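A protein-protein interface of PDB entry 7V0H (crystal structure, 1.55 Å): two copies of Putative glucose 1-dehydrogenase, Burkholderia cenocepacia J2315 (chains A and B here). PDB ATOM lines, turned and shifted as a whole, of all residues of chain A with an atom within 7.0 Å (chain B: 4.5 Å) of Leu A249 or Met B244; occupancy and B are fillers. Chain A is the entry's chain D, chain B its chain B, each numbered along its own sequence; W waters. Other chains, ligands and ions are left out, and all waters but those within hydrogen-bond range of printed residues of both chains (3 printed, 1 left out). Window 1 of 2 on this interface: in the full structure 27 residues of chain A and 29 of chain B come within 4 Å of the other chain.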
ATOM      1  N   ASN A 188     -17.080 -17.094  -8.661  1.00  0.00           N
ATOM      2  CA  ASN A 188     -18.445 -17.553  -8.856  1.00  0.00           C
ATOM      3  C   ASN A 188     -19.056 -16.776 -10.002  1.00  0.00           C
ATOM      4  O   ASN A 188     -18.566 -15.705 -10.374  1.00  0.00           O
ATOM      5  CB  ASN A 188     -19.310 -17.359  -7.597  1.00  0.00           C
ATOM      6  CG  ASN A 188     -18.873 -18.257  -6.460  1.00  0.00           C
ATOM      7  OD1 ASN A 188     -19.121 -19.473  -6.483  1.00  0.00           O
ATOM      8  ND2 ASN A 188     -18.195 -17.675  -5.465  1.00  0.00           N
ATOM      9  N   ALA A 189     -20.104 -17.343 -10.580  1.00  0.00           N
ATOM     10  CA  ALA A 189     -20.860 -16.680 -11.645  1.00  0.00           C
ATOM     11  C   ALA A 189     -22.279 -16.387 -11.192  1.00  0.00           C
ATOM     12  O   ALA A 189     -22.862 -17.121 -10.395  1.00  0.00           O
ATOM     13  CB  ALA A 189     -20.923 -17.543 -12.942  1.00  0.00           C
ATOM     14  N   ILE A 190     -22.842 -15.299 -11.721  1.00  0.00           N
ATOM     15  CA  ILE A 190     -24.282 -15.059 -11.684  1.00  0.00           C
ATOM     16  C   ILE A 190     -24.787 -15.218 -13.107  1.00  0.00           C
ATOM     17  O   ILE A 190     -24.152 -14.727 -14.044  1.00  0.00           O
ATOM     18  CB  ILE A 190     -24.618 -13.664 -11.144  1.00  0.00           C
ATOM     19  CG1 ILE A 190     -24.059 -13.506  -9.729  1.00  0.00           C
ATOM     20  CG2 ILE A 190     -26.166 -13.426 -11.171  1.00  0.00           C
ATOM     21  CD1 ILE A 190     -24.247 -12.084  -9.165  1.00  0.00           C
ATOM     22  N   ASN A 191     -25.896 -15.935 -13.273  1.00  0.00           N
ATOM     23  CA  ASN A 191     -26.478 -16.202 -14.595  1.00  0.00           C
ATOM     24  C   ASN A 191     -27.845 -15.536 -14.622  1.00  0.00           C
ATOM     25  O   ASN A 191     -28.851 -16.171 -14.260  1.00  0.00           O
ATOM     26  CB  ASN A 191     -26.575 -17.705 -14.838  1.00  0.00           C
ATOM     27  CG  ASN A 191     -25.204 -18.350 -14.878  1.00  0.00           C
ATOM     28  OD1 ASN A 191     -24.515 -18.394 -13.864  1.00  0.00           O
ATOM     29  ND2 ASN A 191     -24.781 -18.812 -16.052  1.00  0.00           N
ATOM     30  N   PRO A 192     -27.930 -14.249 -14.983  1.00  0.00           N
ATOM     31  CA  PRO A 192     -29.234 -13.564 -14.934  1.00  0.00           C
ATOM     32  C   PRO A 192     -30.187 -14.071 -16.000  1.00  0.00           C
ATOM     33  O   PRO A 192     -29.775 -14.493 -17.085  1.00  0.00           O
ATOM     34  CB  PRO A 192     -28.889 -12.089 -15.201  1.00  0.00           C
ATOM     35  CG  PRO A 192     -27.389 -11.972 -14.843  1.00  0.00           C
ATOM     36  CD  PRO A 192     -26.827 -13.317 -15.282  1.00  0.00           C
ATOM     37  N   LEU A 220     -41.925 -16.696 -11.304  1.00  0.00           N
ATOM     38  CA  LEU A 220     -42.268 -15.560 -10.453  1.00  0.00           C
ATOM     39  C   LEU A 220     -42.896 -14.404 -11.225  1.00  0.00           C
ATOM     40  O   LEU A 220     -43.146 -13.346 -10.634  1.00  0.00           O
ATOM     41  CB  LEU A 220     -41.023 -15.090  -9.681  1.00  0.00           C
ATOM     42  CG  LEU A 220     -40.535 -16.116  -8.655  1.00  0.00           C
ATOM     43  CD1 LEU A 220     -39.241 -15.628  -8.022  1.00  0.00           C
ATOM     44  CD2 LEU A 220     -41.584 -16.337  -7.558  1.00  0.00           C
ATOM     45  N   ASP A 228     -32.317  -6.904  -8.881  1.00  0.00           N
ATOM     46  CA  ASP A 228     -32.460  -8.342  -8.654  1.00  0.00           C
ATOM     47  C   ASP A 228     -31.116  -9.051  -8.712  1.00  0.00           C
ATOM     48  O   ASP A 228     -30.907 -10.066  -8.031  1.00  0.00           O
ATOM     49  CB  ASP A 228     -33.408  -8.946  -9.702  1.00  0.00           C
ATOM     50  CG  ASP A 228     -34.853  -8.522  -9.498  1.00  0.00           C
ATOM     51  OD1 ASP A 228     -35.314  -8.434  -8.338  1.00  0.00           O
ATOM     52  OD2 ASP A 228     -35.529  -8.277 -10.522  1.00  0.00           O
ATOM     53  N   ILE A 229     -30.215  -8.566  -9.561  1.00  0.00           N
ATOM     54  CA  ILE A 229     -28.874  -9.129  -9.677  1.00  0.00           C
ATOM     55  C   ILE A 229     -27.934  -8.513  -8.660  1.00  0.00           C
ATOM     56  O   ILE A 229     -27.077  -9.201  -8.098  1.00  0.00           O
ATOM     57  CB  ILE A 229     -28.335  -8.919 -11.101  1.00  0.00           C
ATOM     58  CG1 ILE A 229     -29.346  -9.420 -12.134  1.00  0.00           C
ATOM     59  CG2 ILE A 229     -27.008  -9.635 -11.268  1.00  0.00           C
ATOM     60  CD1 ILE A 229     -29.843 -10.853 -11.899  1.00  0.00           C
ATOM     61  N   VAL A 232     -27.644 -10.186  -5.274  1.00  0.00           N
ATOM     62  CA  VAL A 232     -26.921 -11.454  -5.300  1.00  0.00           C
ATOM     63  C   VAL A 232     -25.417 -11.206  -5.425  1.00  0.00           C
ATOM     64  O   VAL A 232     -24.600 -11.925  -4.829  1.00  0.00           O
ATOM     65  CB  VAL A 232     -27.458 -12.343  -6.431  1.00  0.00           C
ATOM     66  CG1 VAL A 232     -26.731 -13.699  -6.451  1.00  0.00           C
ATOM     67  CG2 VAL A 232     -28.957 -12.529  -6.240  1.00  0.00           C
ATOM     68  N   PHE A 235     -24.095 -10.471  -1.977  1.00  0.00           N
ATOM     69  CA  PHE A 235     -23.946 -11.729  -1.246  1.00  0.00           C
ATOM     70  C   PHE A 235     -22.658 -12.448  -1.637  1.00  0.00           C
ATOM     71  O   PHE A 235     -21.856 -12.831  -0.769  1.00  0.00           O
ATOM     72  CB  PHE A 235     -25.173 -12.613  -1.506  1.00  0.00           C
ATOM     73  CG  PHE A 235     -24.954 -14.061  -1.173  1.00  0.00           C
ATOM     74  CD1 PHE A 235     -24.808 -14.474   0.164  1.00  0.00           C
ATOM     75  CD2 PHE A 235     -24.875 -15.001  -2.180  1.00  0.00           C
ATOM     76  CE1 PHE A 235     -24.590 -15.841   0.478  1.00  0.00           C
ATOM     77  CE2 PHE A 235     -24.646 -16.362  -1.868  1.00  0.00           C
ATOM     78  CZ  PHE A 235     -24.518 -16.760  -0.526  1.00  0.00           C
ATOM     79  N   LEU A 236     -22.422 -12.616  -2.945  1.00  0.00           N
ATOM     80  CA  LEU A 236     -21.235 -13.351  -3.363  1.00  0.00           C
ATOM     81  C   LEU A 236     -19.951 -12.613  -3.017  1.00  0.00           C
ATOM     82  O   LEU A 236     -18.907 -13.253  -2.818  1.00  0.00           O
ATOM     83  CB  LEU A 236     -21.281 -13.614  -4.872  1.00  0.00           C
ATOM     84  CG  LEU A 236     -22.267 -14.675  -5.332  1.00  0.00           C
ATOM     85  CD1 LEU A 236     -22.277 -14.709  -6.863  1.00  0.00           C
ATOM     86  CD2 LEU A 236     -21.803 -16.036  -4.789  1.00  0.00           C
ATOM     87  N   MET A 244     -18.693 -20.828  -0.757  1.00  0.00           N
ATOM     88  CA  MET A 244     -19.140 -21.046  -2.132  1.00  0.00           C
ATOM     89  C   MET A 244     -18.046 -20.608  -3.103  1.00  0.00           C
ATOM     90  O   MET A 244     -17.685 -19.427  -3.144  1.00  0.00           O
ATOM     91  CB  MET A 244     -20.426 -20.258  -2.404  1.00  0.00           C
ATOM     92  CG  MET A 244     -21.618 -20.788  -1.614  1.00  0.00           C
ATOM     93  SD  MET A 244     -23.130 -19.913  -2.047  1.00  0.00           S
ATOM     94  CE  MET A 244     -22.925 -19.770  -3.812  1.00  0.00           C
ATOM     95  N   GLY A 246     -16.920 -21.599  -7.439  1.00  0.00           N
ATOM     96  CA  GLY A 246     -17.225 -22.425  -8.601  1.00  0.00           C
ATOM     97  C   GLY A 246     -18.697 -22.594  -8.872  1.00  0.00           C
ATOM     98  O   GLY A 246     -19.062 -23.474  -9.672  1.00  0.00           O
ATOM     99  N   GLU A 247     -19.543 -21.799  -8.228  1.00  0.00           N
ATOM    100  CA  GLU A 247     -20.981 -21.869  -8.425  1.00  0.00           C
ATOM    101  C   GLU A 247     -21.447 -20.947  -9.547  1.00  0.00           C
ATOM    102  O   GLU A 247     -20.769 -19.993  -9.927  1.00  0.00           O
ATOM    103  CB  GLU A 247     -21.717 -21.514  -7.135  1.00  0.00           C
ATOM    104  CG  GLU A 247     -21.687 -22.676  -6.135  1.00  0.00           C
ATOM    105  CD  GLU A 247     -22.386 -23.918  -6.688  1.00  0.00           C
ATOM    106  OE1 GLU A 247     -23.664 -23.951  -6.681  1.00  0.00           O
ATOM    107  OE2 GLU A 247     -21.645 -24.839  -7.152  1.00  0.00           O
ATOM    108  N   HIS A 248     -22.627 -21.271 -10.094  1.00  0.00           N
ATOM    109  CA  HIS A 248     -23.274 -20.500 -11.153  1.00  0.00           C
ATOM    110  C   HIS A 248     -24.695 -20.260 -10.655  1.00  0.00           C
ATOM    111  O   HIS A 248     -25.520 -21.182 -10.637  1.00  0.00           O
ATOM    112  CB  HIS A 248     -23.253 -21.247 -12.481  1.00  0.00           C
ATOM    113  CG  HIS A 248     -21.880 -21.669 -12.899  1.00  0.00           C
ATOM    114  ND1 HIS A 248     -21.235 -22.767 -12.352  1.00  0.00           N
ATOM    115  CD2 HIS A 248     -21.030 -21.159 -13.829  1.00  0.00           C
ATOM    116  CE1 HIS A 248     -20.038 -22.880 -12.900  1.00  0.00           C
ATOM    117  NE2 HIS A 248     -19.895 -21.924 -13.803  1.00  0.00           N
ATOM    118  N   LEU A 249     -24.961 -19.058 -10.170  1.00  0.00           N
ATOM    119  CA  LEU A 249     -26.238 -18.771  -9.514  1.00  0.00           C
ATOM    120  C   LEU A 249     -27.209 -18.237 -10.561  1.00  0.00           C
ATOM    121  O   LEU A 249     -27.027 -17.124 -11.067  1.00  0.00           O
ATOM    122  CB  LEU A 249     -26.045 -17.765  -8.380  1.00  0.00           C
ATOM    123  CG  LEU A 249     -25.372 -18.303  -7.094  1.00  0.00           C
ATOM    124  CD1 LEU A 249     -23.906 -18.646  -7.241  1.00  0.00           C
ATOM    125  CD2 LEU A 249     -25.512 -17.261  -6.002  1.00  0.00           C
ATOM    126  N   VAL A 250     -28.253 -19.012 -10.866  1.00  0.00           N
ATOM    127  CA  VAL A 250     -29.236 -18.567 -11.848  1.00  0.00           C
ATOM    128  C   VAL A 250     -30.206 -17.637 -11.140  1.00  0.00           C
ATOM    129  O   VAL A 250     -30.827 -18.004 -10.134  1.00  0.00           O
ATOM    130  CB  VAL A 250     -29.975 -19.745 -12.489  1.00  0.00           C
ATOM    131  CG1 VAL A 250     -31.094 -19.212 -13.385  1.00  0.00           C
ATOM    132  CG2 VAL A 250     -29.028 -20.599 -13.280  1.00  0.00           C
ATOM    133  N   VAL A 251     -30.311 -16.408 -11.645  1.00  0.00           N
ATOM    134  CA  VAL A 251     -31.107 -15.369 -11.007  1.00  0.00           C
ATOM    135  C   VAL A 251     -32.049 -14.853 -12.083  1.00  0.00           C
ATOM    136  O   VAL A 251     -31.779 -13.839 -12.740  1.00  0.00           O
ATOM    137  CB  VAL A 251     -30.231 -14.244 -10.414  1.00  0.00           C
ATOM    138  CG1 VAL A 251     -31.126 -13.261  -9.645  1.00  0.00           C
ATOM    139  CG2 VAL A 251     -29.181 -14.843  -9.468  1.00  0.00           C
ATOM    140  N   SER A 252     -33.163 -15.574 -12.263  1.00  0.00           N
ATOM    141  CA  SER A 252     -34.010 -15.431 -13.441  1.00  0.00           C
ATOM    142  C   SER A 252     -35.478 -15.494 -13.065  1.00  0.00           C
ATOM    143  O   SER A 252     -36.339 -15.616 -13.963  1.00  0.00           O
ATOM    144  CB  SER A 252     -33.705 -16.558 -14.423  1.00  0.00           C
ATOM    145  OG  SER A 252     -34.085 -17.783 -13.818  1.00  0.00           O
ATOM    146  N   GLY A 253     -35.792 -15.469 -11.767  1.00  0.00           N
ATOM    147  CA  GLY A 253     -37.162 -15.664 -11.354  1.00  0.00           C
ATOM    148  C   GLY A 253     -37.638 -17.083 -11.544  1.00  0.00           C
ATOM    149  O   GLY A 253     -38.854 -17.318 -11.568  1.00  0.00           O
ATOM    150  N   GLY A 254     -36.719 -18.040 -11.699  1.00  0.00           N
ATOM    151  CA  GLY A 254     -37.098 -19.439 -11.778  1.00  0.00           C
ATOM    152  C   GLY A 254     -37.007 -20.077 -13.146  1.00  0.00           C
ATOM    153  O   GLY A 254     -37.303 -21.267 -13.261  1.00  0.00           O
ATOM    154  N   ARG B 186     -40.972 -18.665  -3.020  1.00  0.00           N
ATOM    155  CA  ARG B 186     -39.710 -19.173  -3.557  1.00  0.00           C
ATOM    156  C   ARG B 186     -39.343 -20.482  -2.889  1.00  0.00           C
ATOM    157  O   ARG B 186     -39.635 -20.690  -1.703  1.00  0.00           O
ATOM    158  CB  ARG B 186     -38.589 -18.151  -3.355  1.00  0.00           C
ATOM    159  CG  ARG B 186     -38.863 -16.824  -4.094  1.00  0.00           C
ATOM    160  CD  ARG B 186     -37.684 -15.850  -4.030  1.00  0.00           C
ATOM    161  NE  ARG B 186     -37.516 -15.309  -2.683  1.00  0.00           N
ATOM    162  CZ  ARG B 186     -36.594 -15.719  -1.816  1.00  0.00           C
ATOM    163  NH1 ARG B 186     -35.683 -16.635  -2.139  1.00  0.00           N
ATOM    164  NH2 ARG B 186     -36.586 -15.198  -0.590  1.00  0.00           N
ATOM    165  N   ASN B 188     -35.946 -23.124  -2.778  1.00  0.00           N
ATOM    166  CA  ASN B 188     -34.562 -23.317  -3.189  1.00  0.00           C
ATOM    167  C   ASN B 188     -33.933 -24.359  -2.282  1.00  0.00           C
ATOM    168  O   ASN B 188     -34.426 -24.628  -1.186  1.00  0.00           O
ATOM    169  CB  ASN B 188     -33.726 -22.034  -3.096  1.00  0.00           C
ATOM    170  CG  ASN B 188     -34.160 -20.968  -4.106  1.00  0.00           C
ATOM    171  OD1 ASN B 188     -33.803 -21.030  -5.290  1.00  0.00           O
ATOM    172  ND2 ASN B 188     -34.869 -19.942  -3.623  1.00  0.00           N
ATOM    173  N   PHE B 235     -29.327 -15.627   3.421  1.00  0.00           N
ATOM    174  CA  PHE B 235     -29.470 -15.049   2.086  1.00  0.00           C
ATOM    175  C   PHE B 235     -30.744 -15.533   1.391  1.00  0.00           C
ATOM    176  O   PHE B 235     -31.552 -14.724   0.914  1.00  0.00           O
ATOM    177  CB  PHE B 235     -28.218 -15.387   1.262  1.00  0.00           C
ATOM    178  CG  PHE B 235     -28.393 -15.170  -0.206  1.00  0.00           C
ATOM    179  CD1 PHE B 235     -28.520 -13.873  -0.723  1.00  0.00           C
ATOM    180  CD2 PHE B 235     -28.432 -16.259  -1.056  1.00  0.00           C
ATOM    181  CE1 PHE B 235     -28.705 -13.676  -2.097  1.00  0.00           C
ATOM    182  CE2 PHE B 235     -28.618 -16.058  -2.442  1.00  0.00           C
ATOM    183  CZ  PHE B 235     -28.742 -14.757  -2.945  1.00  0.00           C
ATOM    184  N   ALA B 241     -32.539 -12.600  -2.127  1.00  0.00           N
ATOM    185  CA  ALA B 241     -32.726 -13.712  -3.041  1.00  0.00           C
ATOM    186  C   ALA B 241     -34.093 -13.683  -3.722  1.00  0.00           C
ATOM    187  O   ALA B 241     -34.536 -14.720  -4.213  1.00  0.00           O
ATOM    188  CB  ALA B 241     -32.523 -15.038  -2.293  1.00  0.00           C
ATOM    189  N   ARG B 242     -34.735 -12.510  -3.811  1.00  0.00           N
ATOM    190  CA  ARG B 242     -36.108 -12.426  -4.315  1.00  0.00           C
ATOM    191  C   ARG B 242     -36.244 -12.913  -5.748  1.00  0.00           C
ATOM    192  O   ARG B 242     -37.359 -13.264  -6.165  1.00  0.00           O
ATOM    193  CB  ARG B 242     -36.627 -10.985  -4.214  1.00  0.00           C
ATOM    194  CG  ARG B 242     -35.883  -9.974  -5.076  1.00  0.00           C
ATOM    195  CD  ARG B 242     -36.185  -8.549  -4.613  1.00  0.00           C
ATOM    196  NE  ARG B 242     -35.419  -7.529  -5.321  1.00  0.00           N
ATOM    197  CZ  ARG B 242     -34.177  -7.168  -5.010  1.00  0.00           C
ATOM    198  NH1 ARG B 242     -33.482  -7.794  -4.065  1.00  0.00           N
ATOM    199  NH2 ARG B 242     -33.612  -6.157  -5.662  1.00  0.00           N
ATOM    200  N   TRP B 243     -35.157 -12.933  -6.523  1.00  0.00           N
ATOM    201  CA  TRP B 243     -35.265 -13.326  -7.924  1.00  0.00           C
ATOM    202  C   TRP B 243     -34.643 -14.704  -8.173  1.00  0.00           C
ATOM    203  O   TRP B 243     -34.320 -15.062  -9.317  1.00  0.00           O
ATOM    204  CB  TRP B 243     -34.659 -12.223  -8.804  1.00  0.00           C
ATOM    205  CG  TRP B 243     -35.191 -12.233 -10.202  1.00  0.00           C
ATOM    206  CD1 TRP B 243     -34.465 -12.219 -11.363  1.00  0.00           C
ATOM    207  CD2 TRP B 243     -36.567 -12.279 -10.586  1.00  0.00           C
ATOM    208  NE1 TRP B 243     -35.306 -12.257 -12.447  1.00  0.00           N
ATOM    209  CE2 TRP B 243     -36.600 -12.282 -11.996  1.00  0.00           C
ATOM    210  CE3 TRP B 243     -37.775 -12.306  -9.876  1.00  0.00           C
ATOM    211  CZ2 TRP B 243     -37.777 -12.327 -12.710  1.00  0.00           C
ATOM    212  CZ3 TRP B 243     -38.943 -12.339 -10.589  1.00  0.00           C
ATOM    213  CH2 TRP B 243     -38.936 -12.370 -11.994  1.00  0.00           C
ATOM    214  N   MET B 244     -34.457 -15.482  -7.112  1.00  0.00           N
ATOM    215  CA  MET B 244     -33.916 -16.839  -7.200  1.00  0.00           C
ATOM    216  C   MET B 244     -34.960 -17.824  -6.708  1.00  0.00           C
ATOM    217  O   MET B 244     -35.383 -17.756  -5.552  1.00  0.00           O
ATOM    218  CB  MET B 244     -32.646 -16.993  -6.364  1.00  0.00           C
ATOM    219  CG  MET B 244     -31.488 -16.262  -6.923  1.00  0.00           C
ATOM    220  SD  MET B 244     -29.999 -16.532  -5.950  1.00  0.00           S
ATOM    221  CE  MET B 244     -29.547 -18.162  -6.505  1.00  0.00           C
ATOM    222  N   THR B 245     -35.354 -18.747  -7.577  1.00  0.00           N
ATOM    223  CA  THR B 245     -36.206 -19.849  -7.163  1.00  0.00           C
ATOM    224  C   THR B 245     -35.879 -21.045  -8.041  1.00  0.00           C
ATOM    225  O   THR B 245     -35.516 -20.893  -9.215  1.00  0.00           O
ATOM    226  CB  THR B 245     -37.698 -19.475  -7.185  1.00  0.00           C
ATOM    227  OG1 THR B 245     -38.454 -20.471  -6.474  1.00  0.00           O
ATOM    228  CG2 THR B 245     -38.296 -19.361  -8.592  1.00  0.00           C
ATOM    229  N   GLU B 247     -33.289 -22.961  -7.399  1.00  0.00           N
ATOM    230  CA  GLU B 247     -31.846 -23.133  -7.424  1.00  0.00           C
ATOM    231  C   GLU B 247     -31.400 -24.182  -6.420  1.00  0.00           C
ATOM    232  O   GLU B 247     -32.133 -24.549  -5.496  1.00  0.00           O
ATOM    233  CB  GLU B 247     -31.126 -21.822  -7.138  1.00  0.00           C
ATOM    234  CG  GLU B 247     -31.071 -20.913  -8.376  1.00  0.00           C
ATOM    235  CD  GLU B 247     -30.317 -21.539  -9.528  1.00  0.00           C
ATOM    236  OE1 GLU B 247     -29.023 -21.512  -9.480  1.00  0.00           O
ATOM    237  OE2 GLU B 247     -31.030 -22.077 -10.451  1.00  0.00           O
ATOM    238  N   LEU B 249     -27.875 -24.517  -4.351  1.00  0.00           N
ATOM    239  CA  LEU B 249     -26.632 -23.798  -4.087  1.00  0.00           C
ATOM    240  C   LEU B 249     -25.670 -24.779  -3.432  1.00  0.00           C
ATOM    241  O   LEU B 249     -25.909 -25.214  -2.295  1.00  0.00           O
ATOM    242  CB  LEU B 249     -26.901 -22.600  -3.176  1.00  0.00           C
ATOM    243  CG  LEU B 249     -27.553 -21.357  -3.802  1.00  0.00           C
ATOM    244  CD1 LEU B 249     -28.969 -21.588  -4.262  1.00  0.00           C
ATOM    245  CD2 LEU B 249     -27.526 -20.169  -2.836  1.00  0.00           C
HETATM  246  O   HOH W   1     -36.041  -6.045  -7.713  1.00  0.00           O
HETATM  247  O   HOH W   2     -32.474 -11.714  -6.154  1.00  0.00           O
HETATM  248  O   HOH W   3     -37.544 -22.567 -10.868  1.00  0.00           O
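Pro A192 touches none of the printed residues of chain B. Of the printed residues of chain B, Leu A249 touches Met B244 and Glu B247. Printed residues of chain B within 4 Å of Gly A254: Thr B245 (3.3 Å). Asn B188 touches none of the printed residues of chain A. Printed residues of chain A within 4 Å of Phe B235: Val A232 (3.98 Å) and Phe A235 (3.6 Å). Of the printed residues of chain A, Met B244 touches Leu A249, Val A250 and Val A251. Of the printed residues of chain A, Glu B247 touches His A248, Leu A249 and Val A250. The nearest printed residue of chain B that does not touch Leu A249 is Leu B249 (4.7 Å). The nearest printed residue of chain A that does not touch Thr B245 is Val A250 (5.3 Å).
Phe A235 touches its own counterpart, Phe B235. Glu A247 touches Leu B249, and with the chains exchanged Leu A249 touches Glu B247. Leu A249 touches Met B244, but with the chains exchanged Met A244 does not touch Leu B249 (4.5 Å). Positions printed for both chains: 188, 235, 244, 247 and 249. Of the 19 pairs that touch across the chains among the printed residues, 3 have their exchanged pair printed and touching as well.
The backbone carbonyl oxygen (O) of Asn A191 is in hydrogen-bond range of the backbone NH (N) of Val A251. N of Leu A249 is in hydrogen-bond range of O of Ala A189, 2.9 Å away. N of Leu A220 is in hydrogen-bond range of O of Gly A253 (3.1 Å). The side-chain amide oxygen (OD1) of Asn B188 sits at hydrogen-bond distance from the backbone NH (N) of Glu B247 (2.9 Å). O of Met B244 lies within hydrogen-bond range of ND2 of Asn B188 (3.0 Å). The backbone carbonyl oxygen (O) of Glu A247 is in hydrogen-bond range of the backbone NH (N) of Ala A189, at 2.8 Å.
Hydrophobic or aromatic side chains of chain B that line the printed part of chain A: Phe B235, Trp B243 and Met B244. Printed residues of chain A that touch a printed residue of chain B: Leu A220, Asp A228, Val A232, Phe A235, Glu A247, His A248, Leu A249, Val A250, Val A251, Ser A252, Gly A253 and Gly A254. Hydrophobic or aromatic side chains of chain A that line the printed part of chain B: Leu A220, Val A232, Phe A235, Leu A249, Val A250 and Val A251. Among the printed residues, 19 pairs touch across the chains. Among the printed residues, Asp or Glu carboxylates within 4 Å of a Lys or Arg side-chain nitrogen of the other chain: Asp A228 with Arg B242 (3.2 Å).
Trp B243 touches Asp A228 (CB to CB, 3.6 Å). Val A232 touches Phe B235 (CG2 to CZ, 3.98 Å). Phe A235 touches Phe B235. His A248 touches Glu B247. Leu A249 touches Met B244. Leu A249 touches Glu B247. Met B244 touches Val A250 (CG to O, 3.7 Å). Val A251 touches Trp B243 (O to CD1, 3.4 Å). O of Gly A253 touches CG2 of Thr B245, 3.7 Å away. Gly A254 touches Thr B245 (CA to O, 3.3 Å).
The guanidinium group of Arg B242 is in salt-bridge range of the side-chain carboxylate of Asp A228. N of Val A250 lies within hydrogen-bond range of OE1 of Glu B247 (3.0 Å). O of Trp B243 is in hydrogen-bond range of N of Gly A253 (2.9 Å). The backbone NH of Ser A252 sits at hydrogen-bond distance from the backbone carbonyl oxygen of Trp B243 (3.2 Å).
Water W1 bridges the side-chain carboxylate of Asp A228 (2.6 Å) and the guanidinium group of Arg B242 (2.9 Å). Water W3 bridges O of Gly A254 and O of Thr B245. Water W2 lies within hydrogen-bond range of O of Asp A228 (2.9 Å), N of Trp B243 (3.0 Å) and N of Arg B242 (3.4 Å).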
